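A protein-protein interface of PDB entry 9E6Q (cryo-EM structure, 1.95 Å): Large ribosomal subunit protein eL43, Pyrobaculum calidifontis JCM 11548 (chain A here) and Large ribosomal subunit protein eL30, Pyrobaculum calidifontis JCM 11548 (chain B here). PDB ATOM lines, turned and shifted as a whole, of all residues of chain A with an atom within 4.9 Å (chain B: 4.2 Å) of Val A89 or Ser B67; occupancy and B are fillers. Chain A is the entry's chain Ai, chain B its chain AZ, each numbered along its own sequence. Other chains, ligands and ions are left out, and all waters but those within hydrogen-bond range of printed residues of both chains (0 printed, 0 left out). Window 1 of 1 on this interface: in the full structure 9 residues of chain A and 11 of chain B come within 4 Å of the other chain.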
ATOM      1  N   ARG A  44      23.427  27.629  18.569  1.00  0.00           N
ATOM      2  CA  ARG A  44      22.118  28.120  18.991  1.00  0.00           C
ATOM      3  C   ARG A  44      21.684  29.388  18.271  1.00  0.00           C
ATOM      4  O   ARG A  44      20.749  30.049  18.720  1.00  0.00           O
ATOM      5  CB  ARG A  44      22.064  28.357  20.501  1.00  0.00           C
ATOM      6  CG  ARG A  44      22.457  27.151  21.321  1.00  0.00           C
ATOM      7  CD  ARG A  44      21.476  26.023  21.121  1.00  0.00           C
ATOM      8  NE  ARG A  44      21.709  24.919  22.042  1.00  0.00           N
ATOM      9  CZ  ARG A  44      21.407  24.936  23.332  1.00  0.00           C
ATOM     10  NH1 ARG A  44      20.848  25.993  23.897  1.00  0.00           N
ATOM     11  NH2 ARG A  44      21.664  23.863  24.073  1.00  0.00           N
ATOM     12  N   LEU A  86      26.307  18.037  22.912  1.00  0.00           N
ATOM     13  CA  LEU A  86      25.607  19.248  22.505  1.00  0.00           C
ATOM     14  C   LEU A  86      24.631  19.766  23.549  1.00  0.00           C
ATOM     15  O   LEU A  86      24.211  20.924  23.456  1.00  0.00           O
ATOM     16  CB  LEU A  86      24.846  19.015  21.194  1.00  0.00           C
ATOM     17  CG  LEU A  86      25.665  18.638  19.960  1.00  0.00           C
ATOM     18  CD1 LEU A  86      25.100  17.387  19.313  1.00  0.00           C
ATOM     19  CD2 LEU A  86      25.697  19.781  18.973  1.00  0.00           C
ATOM     20  N   LYS A  87      24.241  18.946  24.522  1.00  0.00           N
ATOM     21  CA  LYS A  87      23.381  19.413  25.608  1.00  0.00           C
ATOM     22  C   LYS A  87      24.231  19.871  26.795  1.00  0.00           C
ATOM     23  O   LYS A  87      24.029  19.472  27.939  1.00  0.00           O
ATOM     24  CB  LYS A  87      22.401  18.320  26.019  1.00  0.00           C
ATOM     25  CG  LYS A  87      21.556  17.772  24.881  1.00  0.00           C
ATOM     26  CD  LYS A  87      20.682  18.847  24.260  1.00  0.00           C
ATOM     27  CE  LYS A  87      19.458  19.114  25.102  1.00  0.00           C
ATOM     28  NZ  LYS A  87      18.451  19.914  24.356  1.00  0.00           N
ATOM     29  N   GLY A  88      25.198  20.732  26.500  1.00  0.00           N
ATOM     30  CA  GLY A  88      26.056  21.277  27.532  1.00  0.00           C
ATOM     31  C   GLY A  88      25.424  22.449  28.246  1.00  0.00           C
ATOM     32  O   GLY A  88      25.753  22.737  29.399  1.00  0.00           O
ATOM     33  N   VAL A  89      24.506  23.135  27.568  1.00  0.00           N
ATOM     34  CA  VAL A  89      23.799  24.241  28.201  1.00  0.00           C
ATOM     35  C   VAL A  89      22.869  23.729  29.291  1.00  0.00           C
ATOM     36  O   VAL A  89      22.732  24.360  30.345  1.00  0.00           O
ATOM     37  CB  VAL A  89      23.042  25.060  27.143  1.00  0.00           C
ATOM     38  CG1 VAL A  89      22.159  26.091  27.800  1.00  0.00           C
ATOM     39  CG2 VAL A  89      24.028  25.726  26.202  1.00  0.00           C
ATOM     40  N   GLU A  90      22.225  22.584  29.068  1.00  0.00           N
ATOM     41  CA  GLU A  90      21.298  22.052  30.059  1.00  0.00           C
ATOM     42  C   GLU A  90      22.014  21.406  31.237  1.00  0.00           C
ATOM     43  O   GLU A  90      21.506  21.451  32.360  1.00  0.00           O
ATOM     44  CB  GLU A  90      20.346  21.055  29.402  1.00  0.00           C
ATOM     45  CG  GLU A  90      19.874  21.487  28.025  1.00  0.00           C
ATOM     46  CD  GLU A  90      19.065  22.769  28.053  1.00  0.00           C
ATOM     47  OE1 GLU A  90      18.528  23.118  29.124  1.00  0.00           O
ATOM     48  OE2 GLU A  90      18.970  23.435  27.000  1.00  0.00           O
ATOM     49  N   ALA A  91      23.175  20.794  31.008  1.00  0.00           N
ATOM     50  CA  ALA A  91      23.940  20.235  32.117  1.00  0.00           C
ATOM     51  C   ALA A  91      24.395  21.328  33.075  1.00  0.00           C
ATOM     52  O   ALA A  91      24.360  21.148  34.298  1.00  0.00           O
ATOM     53  CB  ALA A  91      25.138  19.448  31.590  1.00  0.00           C
ATOM     54  N   GLU A  92      24.827  22.471  32.539  1.00  0.00           N
ATOM     55  CA  GLU A  92      25.266  23.569  33.392  1.00  0.00           C
ATOM     56  C   GLU A  92      24.087  24.304  34.018  1.00  0.00           C
ATOM     57  O   GLU A  92      24.178  24.761  35.162  1.00  0.00           O
ATOM     58  CB  GLU A  92      26.134  24.538  32.593  1.00  0.00           C
ATOM     59  CG  GLU A  92      27.391  23.919  32.021  1.00  0.00           C
ATOM     60  CD  GLU A  92      28.435  23.634  33.079  1.00  0.00           C
ATOM     61  OE1 GLU A  92      28.407  24.293  34.139  1.00  0.00           O
ATOM     62  OE2 GLU A  92      29.294  22.758  32.843  1.00  0.00           O
ATOM     63  N   LYS A  93      22.981  24.436  33.285  1.00  0.00           N
ATOM     64  CA  LYS A  93      21.791  25.067  33.847  1.00  0.00           C
ATOM     65  C   LYS A  93      21.246  24.274  35.024  1.00  0.00           C
ATOM     66  O   LYS A  93      20.851  24.854  36.042  1.00  0.00           O
ATOM     67  CB  LYS A  93      20.718  25.221  32.772  1.00  0.00           C
ATOM     68  CG  LYS A  93      20.646  26.601  32.173  1.00  0.00           C
ATOM     69  CD  LYS A  93      19.690  26.658  31.000  1.00  0.00           C
ATOM     70  CE  LYS A  93      19.799  27.989  30.281  1.00  0.00           C
ATOM     71  NZ  LYS A  93      19.033  27.996  29.003  1.00  0.00           N
ATOM     72  N   ALA B  39      31.247  30.302  27.886  1.00  0.00           N
ATOM     73  CA  ALA B  39      29.894  29.817  27.666  1.00  0.00           C
ATOM     74  C   ALA B  39      29.884  28.296  27.578  1.00  0.00           C
ATOM     75  O   ALA B  39      30.877  27.667  27.213  1.00  0.00           O
ATOM     76  CB  ALA B  39      29.313  30.426  26.395  1.00  0.00           C
ATOM     77  N   ALA B  40      28.744  27.704  27.926  1.00  0.00           N
ATOM     78  CA  ALA B  40      28.655  26.250  27.982  1.00  0.00           C
ATOM     79  C   ALA B  40      28.728  25.615  26.601  1.00  0.00           C
ATOM     80  O   ALA B  40      29.223  24.492  26.467  1.00  0.00           O
ATOM     81  CB  ALA B  40      27.370  25.831  28.688  1.00  0.00           C
ATOM     82  N   ASN B  41      28.249  26.299  25.567  1.00  0.00           N
ATOM     83  CA  ASN B  41      28.266  25.756  24.211  1.00  0.00           C
ATOM     84  C   ASN B  41      29.435  26.286  23.399  1.00  0.00           C
ATOM     85  O   ASN B  41      29.331  26.451  22.185  1.00  0.00           O
ATOM     86  CB  ASN B  41      26.946  26.039  23.502  1.00  0.00           C
ATOM     87  CG  ASN B  41      26.739  27.508  23.212  1.00  0.00           C
ATOM     88  OD1 ASN B  41      27.279  28.366  23.896  1.00  0.00           O
ATOM     89  ND2 ASN B  41      25.961  27.800  22.184  1.00  0.00           N
ATOM     90  N   PRO B  65      26.237  29.091  32.716  1.00  0.00           N
ATOM     91  CA  PRO B  65      25.224  28.055  32.486  1.00  0.00           C
ATOM     92  C   PRO B  65      24.338  28.311  31.277  1.00  0.00           C
ATOM     93  O   PRO B  65      23.232  27.775  31.209  1.00  0.00           O
ATOM     94  CB  PRO B  65      24.409  28.059  33.784  1.00  0.00           C
ATOM     95  CG  PRO B  65      24.683  29.348  34.434  1.00  0.00           C
ATOM     96  CD  PRO B  65      25.964  29.897  33.917  1.00  0.00           C
ATOM     97  N   GLY B  66      24.776  29.142  30.334  1.00  0.00           N
ATOM     98  CA  GLY B  66      23.994  29.418  29.148  1.00  0.00           C
ATOM     99  C   GLY B  66      24.840  29.356  27.893  1.00  0.00           C
ATOM    100  O   GLY B  66      26.031  29.050  27.937  1.00  0.00           O
ATOM    101  N   SER B  67      24.195  29.643  26.770  1.00  0.00           N
ATOM    102  CA  SER B  67      24.885  29.711  25.496  1.00  0.00           C
ATOM    103  C   SER B  67      25.643  31.029  25.376  1.00  0.00           C
ATOM    104  O   SER B  67      25.495  31.938  26.192  1.00  0.00           O
ATOM    105  CB  SER B  67      23.896  29.550  24.345  1.00  0.00           C
ATOM    106  OG  SER B  67      23.077  30.697  24.207  1.00  0.00           O
ATOM    107  N   SER B  68      26.479  31.126  24.343  1.00  0.00           N
ATOM    108  CA  SER B  68      27.177  32.381  24.095  1.00  0.00           C
ATOM    109  C   SER B  68      26.199  33.501  23.768  1.00  0.00           C
ATOM    110  O   SER B  68      26.494  34.672  24.015  1.00  0.00           O
ATOM    111  CB  SER B  68      28.194  32.212  22.971  1.00  0.00           C
ATOM    112  OG  SER B  68      27.568  31.816  21.771  1.00  0.00           O
ATOM    113  N   ILE B  69      25.040  33.163  23.207  1.00  0.00           N
ATOM    114  CA  ILE B  69      24.001  34.159  22.985  1.00  0.00           C
ATOM    115  C   ILE B  69      23.421  34.627  24.313  1.00  0.00           C
ATOM    116  O   ILE B  69      23.107  35.809  24.487  1.00  0.00           O
ATOM    117  CB  ILE B  69      22.913  33.586  22.059  1.00  0.00           C
ATOM    118  CG1 ILE B  69      23.490  33.331  20.667  1.00  0.00           C
ATOM    119  CG2 ILE B  69      21.705  34.510  21.996  1.00  0.00           C
ATOM    120  CD1 ILE B  69      22.565  32.584  19.754  1.00  0.00           C
ATOM    121  N   GLU B  70      23.274  33.713  25.268  1.00  0.00           N
ATOM    122  CA  GLU B  70      22.710  34.064  26.563  1.00  0.00           C
ATOM    123  C   GLU B  70      23.708  34.801  27.442  1.00  0.00           C
ATOM    124  O   GLU B  70      23.308  35.646  28.246  1.00  0.00           O
ATOM    125  CB  GLU B  70      22.209  32.808  27.264  1.00  0.00           C
ATOM    126  CG  GLU B  70      20.739  32.552  27.038  1.00  0.00           C
ATOM    127  CD  GLU B  70      20.349  31.118  27.313  1.00  0.00           C
ATOM    128  OE1 GLU B  70      19.146  30.863  27.520  1.00  0.00           O
ATOM    129  OE2 GLU B  70      21.244  30.245  27.322  1.00  0.00           O
ATOM    130  N   LEU B  71      24.999  34.497  27.308  1.00  0.00           N
ATOM    131  CA  LEU B  71      26.013  35.260  28.020  1.00  0.00           C
ATOM    132  C   LEU B  71      26.074  36.697  27.528  1.00  0.00           C
ATOM    133  O   LEU B  71      26.290  37.614  28.324  1.00  0.00           O
ATOM    134  CB  LEU B  71      27.373  34.590  27.872  1.00  0.00           C
ATOM    135  CG  LEU B  71      28.582  35.242  28.535  1.00  0.00           C
ATOM    136  CD1 LEU B  71      28.324  35.522  30.002  1.00  0.00           C
ATOM    137  CD2 LEU B  71      29.788  34.345  28.378  1.00  0.00           C
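The side-chain amino group (NZ) of Lys A93 lies within salt-bridge range of the side-chain carboxylate (OE1) of Glu B70, 3.2 Å away.
The side-chain carboxylate (OE2) of Glu B70 is in hydrogen-bond range of the backbone NH (N) of Ser B67. OG of Ser B67 lies close to N of Ile B69, at 3.3 Å. N of Ala B40 lies within hydrogen-bond range of O of Gly B66, at 3.0 Å. The side-chain amide oxygen of Asn B41 sits at hydrogen-bond distance from the backbone NH of Ser B68 (2.9 Å).
CG of Arg A44 touches ND2 of Asn B41, 3.7 Å away. Arg A44 touches Ile B69. O of Gly A88 touches CB of Ala B40, 3.6 Å away. Ala B40 touches Val A89 (CB to CA, 3.9 Å). CB of Asn B41 touches CG2 of Val A89 (3.99 Å). O of Pro B65 touches O of Val A89, 3.6 Å away. Val A89 touches Ser B67 (CG2 to N, 3.96 Å). Ala B40 touches Glu A92. Pro B65 touches Glu A92 (CB to O, 3.6 Å). Pro B65 touches Lys A93 (O to CG, 3.0 Å).
Printed residues of chain B within 4 Å of Val A89: Ala B40 (3.9 Å), Asn B41 (3.99 Å), Pro B65 (3.6 Å) and Ser B67 (3.96 Å). Printed residues of chain B within 4 Å of Lys A93: Pro B65 (3.0 Å) and Glu B70 (3.2 Å). Of the printed residues of chain A, Ile B69 touches Arg A44. The nearest printed residue of chain B that does not touch Arg A44 is Ser B67 (4.1 Å).
Of the 10 printed residues of chain B, 6 touch a printed residue of chain A. Hydrophobic or aromatic side chains of chain B within 4 Å of the printed part of chain A: Ala B40, Pro B65 and Ile B69. Among the printed residues, 11 pairs touch across the chains. Among the printed residues, Asp or Glu carboxylates within 4 Å of a Lys or Arg side-chain nitrogen of the other chain: Lys A93 with Glu B70 (3.2 Å).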
